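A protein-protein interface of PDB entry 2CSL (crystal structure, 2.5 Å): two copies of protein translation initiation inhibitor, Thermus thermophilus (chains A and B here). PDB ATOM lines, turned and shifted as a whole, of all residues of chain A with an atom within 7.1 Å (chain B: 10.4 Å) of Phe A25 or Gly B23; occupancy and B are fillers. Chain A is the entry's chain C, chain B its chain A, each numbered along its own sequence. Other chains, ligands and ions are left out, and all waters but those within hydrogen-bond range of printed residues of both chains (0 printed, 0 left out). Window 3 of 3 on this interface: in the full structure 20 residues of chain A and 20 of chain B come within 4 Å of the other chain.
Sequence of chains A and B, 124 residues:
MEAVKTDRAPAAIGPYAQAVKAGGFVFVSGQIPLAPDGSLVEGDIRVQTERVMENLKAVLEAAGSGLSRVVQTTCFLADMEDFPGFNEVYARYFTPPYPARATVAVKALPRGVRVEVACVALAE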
ATOM      1  N   VAL A  20       6.257  30.859   7.410  1.00  0.00           N
ATOM      2  CA  VAL A  20       7.143  31.918   7.899  1.00  0.00           C
ATOM      3  C   VAL A  20       7.950  31.431   9.104  1.00  0.00           C
ATOM      4  O   VAL A  20       7.413  30.774   9.991  1.00  0.00           O
ATOM      5  CB  VAL A  20       6.374  33.247   8.291  1.00  0.00           C
ATOM      6  CG1 VAL A  20       4.930  33.185   7.850  1.00  0.00           C
ATOM      7  CG2 VAL A  20       6.493  33.523   9.782  1.00  0.00           C
ATOM      8  N   LYS A  21       9.244  31.738   9.112  1.00  0.00           N
ATOM      9  CA  LYS A  21      10.131  31.365  10.214  1.00  0.00           C
ATOM     10  C   LYS A  21      10.097  32.505  11.233  1.00  0.00           C
ATOM     11  O   LYS A  21      10.256  33.672  10.870  1.00  0.00           O
ATOM     12  CB  LYS A  21      11.564  31.163   9.702  1.00  0.00           C
ATOM     13  CG  LYS A  21      11.672  30.110   8.603  1.00  0.00           C
ATOM     14  CD  LYS A  21      13.086  29.568   8.407  1.00  0.00           C
ATOM     15  CE  LYS A  21      13.997  30.545   7.689  1.00  0.00           C
ATOM     16  NZ  LYS A  21      15.225  29.859   7.193  1.00  0.00           N
ATOM     17  N   ALA A  22       9.875  32.182  12.501  1.00  0.00           N
ATOM     18  CA  ALA A  22       9.820  33.218  13.528  1.00  0.00           C
ATOM     19  C   ALA A  22       9.857  32.639  14.934  1.00  0.00           C
ATOM     20  O   ALA A  22       9.298  31.573  15.186  1.00  0.00           O
ATOM     21  CB  ALA A  22       8.561  34.052  13.347  1.00  0.00           C
ATOM     22  N   GLY A  23      10.525  33.350  15.840  1.00  0.00           N
ATOM     23  CA  GLY A  23      10.627  32.913  17.222  1.00  0.00           C
ATOM     24  C   GLY A  23      11.089  31.484  17.459  1.00  0.00           C
ATOM     25  O   GLY A  23      10.735  30.873  18.468  1.00  0.00           O
ATOM     26  N   GLY A  24      11.877  30.946  16.536  1.00  0.00           N
ATOM     27  CA  GLY A  24      12.370  29.592  16.691  1.00  0.00           C
ATOM     28  C   GLY A  24      11.454  28.555  16.069  1.00  0.00           C
ATOM     29  O   GLY A  24      11.770  27.366  16.079  1.00  0.00           O
ATOM     30  N   PHE A  25      10.330  28.996  15.510  1.00  0.00           N
ATOM     31  CA  PHE A  25       9.385  28.073  14.892  1.00  0.00           C
ATOM     32  C   PHE A  25       9.121  28.351  13.423  1.00  0.00           C
ATOM     33  O   PHE A  25       9.492  29.390  12.882  1.00  0.00           O
ATOM     34  CB  PHE A  25       8.030  28.106  15.598  1.00  0.00           C
ATOM     35  CG  PHE A  25       8.051  27.589  17.006  1.00  0.00           C
ATOM     36  CD1 PHE A  25       8.377  28.426  18.069  1.00  0.00           C
ATOM     37  CD2 PHE A  25       7.693  26.278  17.274  1.00  0.00           C
ATOM     38  CE1 PHE A  25       8.341  27.964  19.379  1.00  0.00           C
ATOM     39  CE2 PHE A  25       7.656  25.802  18.583  1.00  0.00           C
ATOM     40  CZ  PHE A  25       7.978  26.646  19.638  1.00  0.00           C
ATOM     41  N   VAL A  26       8.457  27.398  12.786  1.00  0.00           N
ATOM     42  CA  VAL A  26       8.079  27.525  11.392  1.00  0.00           C
ATOM     43  C   VAL A  26       6.574  27.330  11.394  1.00  0.00           C
ATOM     44  O   VAL A  26       6.074  26.325  11.897  1.00  0.00           O
ATOM     45  CB  VAL A  26       8.721  26.439  10.509  1.00  0.00           C
ATOM     46  CG1 VAL A  26       8.466  26.748   9.046  1.00  0.00           C
ATOM     47  CG2 VAL A  26      10.202  26.362  10.773  1.00  0.00           C
ATOM     48  N   PHE A  27       5.855  28.304  10.860  1.00  0.00           N
ATOM     49  CA  PHE A  27       4.404  28.230  10.798  1.00  0.00           C
ATOM     50  C   PHE A  27       4.054  27.940   9.348  1.00  0.00           C
ATOM     51  O   PHE A  27       4.241  28.788   8.477  1.00  0.00           O
ATOM     52  CB  PHE A  27       3.808  29.563  11.248  1.00  0.00           C
ATOM     53  CG  PHE A  27       4.074  29.886  12.694  1.00  0.00           C
ATOM     54  CD1 PHE A  27       3.197  29.465  13.688  1.00  0.00           C
ATOM     55  CD2 PHE A  27       5.220  30.580  13.069  1.00  0.00           C
ATOM     56  CE1 PHE A  27       3.454  29.731  15.032  1.00  0.00           C
ATOM     57  CE2 PHE A  27       5.486  30.851  14.411  1.00  0.00           C
ATOM     58  CZ  PHE A  27       4.601  30.423  15.394  1.00  0.00           C
ATOM     59  N   ARG A  69      10.605  17.405  12.594  1.00  0.00           N
ATOM     60  CA  ARG A  69      10.616  18.512  13.541  1.00  0.00           C
ATOM     61  C   ARG A  69       9.255  19.179  13.742  1.00  0.00           C
ATOM     62  O   ARG A  69       9.153  20.243  14.354  1.00  0.00           O
ATOM     63  CB  ARG A  69      11.647  19.536  13.091  1.00  0.00           C
ATOM     64  CG  ARG A  69      13.038  18.943  12.917  1.00  0.00           C
ATOM     65  CD  ARG A  69      14.005  19.498  13.948  1.00  0.00           C
ATOM     66  NE  ARG A  69      14.037  18.731  15.189  1.00  0.00           N
ATOM     67  CZ  ARG A  69      14.477  19.218  16.346  1.00  0.00           C
ATOM     68  NH1 ARG A  69      14.910  20.474  16.414  1.00  0.00           N
ATOM     69  NH2 ARG A  69      14.494  18.449  17.431  1.00  0.00           N
ATOM     70  N   VAL A  71       5.855  19.807  15.473  1.00  0.00           N
ATOM     71  CA  VAL A  71       5.339  19.627  16.825  1.00  0.00           C
ATOM     72  C   VAL A  71       3.815  19.675  16.906  1.00  0.00           C
ATOM     73  O   VAL A  71       3.223  19.205  17.876  1.00  0.00           O
ATOM     74  CB  VAL A  71       5.919  20.686  17.784  1.00  0.00           C
ATOM     75  CG1 VAL A  71       7.424  20.564  17.818  1.00  0.00           C
ATOM     76  CG2 VAL A  71       5.511  22.090  17.342  1.00  0.00           C
ATOM     77  N   VAL A 120       2.958  23.322  12.667  1.00  0.00           N
ATOM     78  CA  VAL A 120       3.970  24.155  13.283  1.00  0.00           C
ATOM     79  C   VAL A 120       5.142  23.242  13.602  1.00  0.00           C
ATOM     80  O   VAL A 120       4.968  22.185  14.216  1.00  0.00           O
ATOM     81  CB  VAL A 120       3.447  24.805  14.573  1.00  0.00           C
ATOM     82  CG1 VAL A 120       4.580  25.501  15.304  1.00  0.00           C
ATOM     83  CG2 VAL A 120       2.351  25.800  14.232  1.00  0.00           C
ATOM     84  N   ALA A 121       6.333  23.637  13.167  1.00  0.00           N
ATOM     85  CA  ALA A 121       7.531  22.838  13.417  1.00  0.00           C
ATOM     86  C   ALA A 121       8.629  23.697  14.011  1.00  0.00           C
ATOM     87  O   ALA A 121       8.557  24.926  13.956  1.00  0.00           O
ATOM     88  CB  ALA A 121       8.020  22.206  12.130  1.00  0.00           C
ATOM     89  N   LEU A 122       9.632  23.042  14.592  1.00  0.00           N
ATOM     90  CA  LEU A 122      10.772  23.738  15.174  1.00  0.00           C
ATOM     91  C   LEU A 122      11.754  24.112  14.077  1.00  0.00           C
ATOM     92  O   LEU A 122      11.998  23.330  13.157  1.00  0.00           O
ATOM     93  CB  LEU A 122      11.500  22.844  16.183  1.00  0.00           C
ATOM     94  CG  LEU A 122      10.902  22.672  17.578  1.00  0.00           C
ATOM     95  CD1 LEU A 122      11.685  21.612  18.349  1.00  0.00           C
ATOM     96  CD2 LEU A 122      10.946  24.009  18.309  1.00  0.00           C
ATOM     97  N   ALA A 123      12.306  25.315  14.173  1.00  0.00           N
ATOM     98  CA  ALA A 123      13.302  25.762  13.217  1.00  0.00           C
ATOM     99  C   ALA A 123      14.571  25.073  13.690  1.00  0.00           C
ATOM    100  O   ALA A 123      14.616  24.591  14.822  1.00  0.00           O
ATOM    101  CB  ALA A 123      13.458  27.270  13.290  1.00  0.00           C
ATOM    102  N   MET B   1      12.711  18.913  21.716  1.00  0.00           N
ATOM    103  CA  MET B   1      11.423  18.268  21.320  1.00  0.00           C
ATOM    104  C   MET B   1      11.249  16.927  22.017  1.00  0.00           C
ATOM    105  O   MET B   1      12.047  16.010  21.830  1.00  0.00           O
ATOM    106  CB  MET B   1      11.375  18.057  19.812  1.00  0.00           C
ATOM    107  CG  MET B   1      10.073  17.456  19.337  1.00  0.00           C
ATOM    108  SD  MET B   1      10.088  17.170  17.444  1.00  0.00           S
ATOM    109  CE  MET B   1      10.588  18.940  16.898  1.00  0.00           C
ATOM    110  N   GLU B   2      10.182  16.809  22.797  1.00  0.00           N
ATOM    111  CA  GLU B   2       9.924  15.594  23.548  1.00  0.00           C
ATOM    112  C   GLU B   2       8.434  15.314  23.689  1.00  0.00           C
ATOM    113  O   GLU B   2       7.654  16.201  24.040  1.00  0.00           O
ATOM    114  CB  GLU B   2      10.571  15.739  24.921  1.00  0.00           C
ATOM    115  CG  GLU B   2      10.148  14.736  25.958  1.00  0.00           C
ATOM    116  CD  GLU B   2      10.743  15.061  27.313  1.00  0.00           C
ATOM    117  OE1 GLU B   2      10.567  16.210  27.778  1.00  0.00           O
ATOM    118  OE2 GLU B   2      11.393  14.175  27.909  1.00  0.00           O
ATOM    119  N   VAL B  20       3.421  17.607  22.853  1.00  0.00           N
ATOM    120  CA  VAL B  20       4.831  17.731  22.536  1.00  0.00           C
ATOM    121  C   VAL B  20       5.428  18.938  23.242  1.00  0.00           C
ATOM    122  O   VAL B  20       4.860  20.033  23.216  1.00  0.00           O
ATOM    123  CB  VAL B  20       5.061  17.893  21.009  1.00  0.00           C
ATOM    124  CG1 VAL B  20       6.523  18.237  20.731  1.00  0.00           C
ATOM    125  CG2 VAL B  20       4.683  16.610  20.284  1.00  0.00           C
ATOM    126  N   LYS B  21       6.571  18.721  23.887  1.00  0.00           N
ATOM    127  CA  LYS B  21       7.282  19.789  24.572  1.00  0.00           C
ATOM    128  C   LYS B  21       8.344  20.298  23.609  1.00  0.00           C
ATOM    129  O   LYS B  21       9.201  19.525  23.183  1.00  0.00           O
ATOM    130  CB  LYS B  21       7.943  19.266  25.855  1.00  0.00           C
ATOM    131  CG  LYS B  21       7.074  19.430  27.094  1.00  0.00           C
ATOM    132  CD  LYS B  21       7.868  19.285  28.382  1.00  0.00           C
ATOM    133  CE  LYS B  21       7.877  17.854  28.886  1.00  0.00           C
ATOM    134  NZ  LYS B  21       8.620  17.730  30.176  1.00  0.00           N
ATOM    135  N   ALA B  22       8.283  21.583  23.256  1.00  0.00           N
ATOM    136  CA  ALA B  22       9.256  22.164  22.324  1.00  0.00           C
ATOM    137  C   ALA B  22       9.324  23.685  22.335  1.00  0.00           C
ATOM    138  O   ALA B  22       8.307  24.362  22.476  1.00  0.00           O
ATOM    139  CB  ALA B  22       8.959  21.699  20.914  1.00  0.00           C
ATOM    140  N   GLY B  23      10.534  24.208  22.169  1.00  0.00           N
ATOM    141  CA  GLY B  23      10.739  25.646  22.128  1.00  0.00           C
ATOM    142  C   GLY B  23      10.096  26.468  23.231  1.00  0.00           C
ATOM    143  O   GLY B  23       9.727  27.625  23.011  1.00  0.00           O
ATOM    144  N   GLY B  24       9.946  25.880  24.412  1.00  0.00           N
ATOM    145  CA  GLY B  24       9.358  26.621  25.512  1.00  0.00           C
ATOM    146  C   GLY B  24       7.866  26.444  25.693  1.00  0.00           C
ATOM    147  O   GLY B  24       7.313  26.853  26.714  1.00  0.00           O
ATOM    148  N   PHE B  25       7.203  25.836  24.718  1.00  0.00           N
ATOM    149  CA  PHE B  25       5.766  25.629  24.821  1.00  0.00           C
ATOM    150  C   PHE B  25       5.393  24.159  24.899  1.00  0.00           C
ATOM    151  O   PHE B  25       6.235  23.273  24.740  1.00  0.00           O
ATOM    152  CB  PHE B  25       5.045  26.251  23.625  1.00  0.00           C
ATOM    153  CG  PHE B  25       5.155  27.743  23.547  1.00  0.00           C
ATOM    154  CD1 PHE B  25       6.212  28.345  22.873  1.00  0.00           C
ATOM    155  CD2 PHE B  25       4.183  28.552  24.133  1.00  0.00           C
ATOM    156  CE1 PHE B  25       6.300  29.728  22.774  1.00  0.00           C
ATOM    157  CE2 PHE B  25       4.258  29.942  24.043  1.00  0.00           C
ATOM    158  CZ  PHE B  25       5.317  30.534  23.361  1.00  0.00           C
ATOM    159  N   VAL B  26       4.115  23.912  25.159  1.00  0.00           N
ATOM    160  CA  VAL B  26       3.586  22.561  25.222  1.00  0.00           C
ATOM    161  C   VAL B  26       2.443  22.554  24.231  1.00  0.00           C
ATOM    162  O   VAL B  26       1.510  23.331  24.383  1.00  0.00           O
ATOM    163  CB  VAL B  26       2.994  22.223  26.586  1.00  0.00           C
ATOM    164  CG1 VAL B  26       2.526  20.778  26.588  1.00  0.00           C
ATOM    165  CG2 VAL B  26       4.012  22.460  27.670  1.00  0.00           C
ATOM    166  N   PHE B  27       2.524  21.701  23.213  1.00  0.00           N
ATOM    167  CA  PHE B  27       1.463  21.620  22.215  1.00  0.00           C
ATOM    168  C   PHE B  27       0.613  20.398  22.549  1.00  0.00           C
ATOM    169  O   PHE B  27       1.085  19.268  22.473  1.00  0.00           O
ATOM    170  CB  PHE B  27       2.068  21.496  20.816  1.00  0.00           C
ATOM    171  CG  PHE B  27       2.902  22.675  20.416  1.00  0.00           C
ATOM    172  CD1 PHE B  27       2.323  23.774  19.783  1.00  0.00           C
ATOM    173  CD2 PHE B  27       4.262  22.714  20.723  1.00  0.00           C
ATOM    174  CE1 PHE B  27       3.085  24.896  19.469  1.00  0.00           C
ATOM    175  CE2 PHE B  27       5.036  23.832  20.414  1.00  0.00           C
ATOM    176  CZ  PHE B  27       4.443  24.929  19.785  1.00  0.00           C
ATOM    177  N   VAL B 120      -2.355  25.195  23.580  1.00  0.00           N
ATOM    178  CA  VAL B 120      -0.920  25.434  23.629  1.00  0.00           C
ATOM    179  C   VAL B 120      -0.676  26.109  24.972  1.00  0.00           C
ATOM    180  O   VAL B 120      -1.403  27.039  25.352  1.00  0.00           O
ATOM    181  CB  VAL B 120      -0.446  26.374  22.497  1.00  0.00           C
ATOM    182  CG1 VAL B 120       1.053  26.594  22.594  1.00  0.00           C
ATOM    183  CG2 VAL B 120      -0.790  25.778  21.156  1.00  0.00           C
ATOM    184  N   ALA B 121       0.327  25.625  25.701  1.00  0.00           N
ATOM    185  CA  ALA B 121       0.654  26.186  27.002  1.00  0.00           C
ATOM    186  C   ALA B 121       2.146  26.438  27.155  1.00  0.00           C
ATOM    187  O   ALA B 121       2.964  25.940  26.370  1.00  0.00           O
ATOM    188  CB  ALA B 121       0.174  25.257  28.102  1.00  0.00           C
ATOM    189  N   LEU B 122       2.488  27.235  28.163  1.00  0.00           N
ATOM    190  CA  LEU B 122       3.879  27.545  28.462  1.00  0.00           C
ATOM    191  C   LEU B 122       4.432  26.399  29.283  1.00  0.00           C
ATOM    192  O   LEU B 122       3.757  25.892  30.177  1.00  0.00           O
ATOM    193  CB  LEU B 122       3.985  28.827  29.287  1.00  0.00           C
ATOM    194  CG  LEU B 122       3.937  30.199  28.622  1.00  0.00           C
ATOM    195  CD1 LEU B 122       3.863  31.253  29.706  1.00  0.00           C
ATOM    196  CD2 LEU B 122       5.166  30.414  27.760  1.00  0.00           C
ATOM    197  N   ALA B 123       5.651  25.981  28.984  1.00  0.00           N
ATOM    198  CA  ALA B 123       6.256  24.903  29.750  1.00  0.00           C
ATOM    199  C   ALA B 123       6.824  25.532  31.014  1.00  0.00           C
ATOM    200  O   ALA B 123       7.304  26.665  30.983  1.00  0.00           O
ATOM    201  CB  ALA B 123       7.359  24.244  28.947  1.00  0.00           C
ATOM    202  N   GLU B 124       6.749  24.817  32.129  1.00  0.00           N
ATOM    203  CA  GLU B 124       7.281  25.342  33.381  1.00  0.00           C
ATOM    204  C   GLU B 124       8.671  24.765  33.651  1.00  0.00           C
ATOM    205  O   GLU B 124       8.787  23.861  34.509  1.00  0.00           O
ATOM    206  CB  GLU B 124       6.340  25.025  34.550  1.00  0.00           C
ATOM    207  CG  GLU B 124       5.053  25.843  34.561  1.00  0.00           C
ATOM    208  CD  GLU B 124       4.183  25.531  35.766  1.00  0.00           C
ATOM    209  OE1 GLU B 124       4.640  25.762  36.906  1.00  0.00           O
ATOM    210  OE2 GLU B 124       3.047  25.046  35.578  1.00  0.00           O
ATOM    211  OXT GLU B 124       9.627  25.221  32.986  1.00  0.00           O
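The backbone carbonyl oxygen (O) of Val B20 lies within hydrogen-bond range of the backbone NH (N) of Phe B27 (2.9 Å). The backbone carbonyl oxygen of Arg A69 is in hydrogen-bond range of the backbone NH of Leu A122 (2.8 Å). N of Val A71 lies within hydrogen-bond range of O of Val A120.
Phe A25 touches Ala B22 (CZ to O, 3.7 Å). Gly B23 touches Phe A25. CZ of Phe B27 touches CE2 of Phe A25, at 3.5 Å. Val A71 touches Met B1 (CG1 to CE, 3.7 Å). CG2 of Val B20 touches O of Val A71, at 3.8 Å. Val A71 touches Ala B22 (CG1 to CB, 3.6 Å). CG2 of Val A71 touches CE2 of Phe B27 (3.6 Å). Leu A122 touches Met B1 (CD1 to CE, 3.2 Å). Ala B22 touches Leu A122. Leu A122 touches Gly B23.
No residue of chain B comes within 4 Å of Gly A23. No residue of chain B comes within 4 Å of Gly A24. Phe A25 touches just these residues of chain B: Ala B22 (3.7 Å), Gly B23 (3.9 Å) and Phe B27 (3.5 Å). Of the printed residues of chain B, Arg A69 touches Met B1. Of chain B, only Met B1 (3.2 Å), Ala B22 (3.7 Å) and Gly B23 (3.9 Å) come within 4 Å of Leu A122. Ala A123 touches none of the printed residues of chain B. Of the printed residues of chain A, Met B1 touches Arg A69 (3.2 Å), Val A71 (3.7 Å) and Leu A122 (3.2 Å). Of the printed residues of chain A, Val B20 touches Val A71 (3.8 Å). Of the printed residues of chain A, Ala B22 touches Phe A25 (3.7 Å), Val A71 (3.6 Å) and Leu A122 (3.7 Å). Gly B23 touches just these residues of chain A: Phe A25 and Leu A122. The nearest residue of chain B that does not touch Phe A25 is Phe B25 (4.1 Å). The nearest residue of chain A that does not touch Gly B23 is Gly A23 (5.7 Å). The nearest printed residue of chain B that does not touch Val A71 is Lys B21 (5.7 Å).
Of the 15 printed residues of chain B, 5 touch a printed residue of chain A. Hydrophobic or aromatic side chains of chain B that line the printed part of chain A: Met B1, Val B20, Ala B22 and Phe B27. Among the printed residues, 11 pairs touch across the chains. Among the printed residues, no Asp or Glu carboxylate lies within 4 Å of a Lys or Arg side-chain nitrogen of the other chain.
Phe A25 touches Ala B22, but with the chains exchanged Ala A22 does not touch Phe B25 (8.4 Å). Phe A25 touches Gly B23, but with the chains exchanged Gly A23 does not touch Phe B25 (6.3 Å). Leu A122 touches Ala B22, but with the chains exchanged Ala A22 does not touch Leu B122 (13.3 Å). Leu A122 touches Gly B23, but with the chains exchanged Gly A23 does not touch Leu B122 (10.8 Å).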
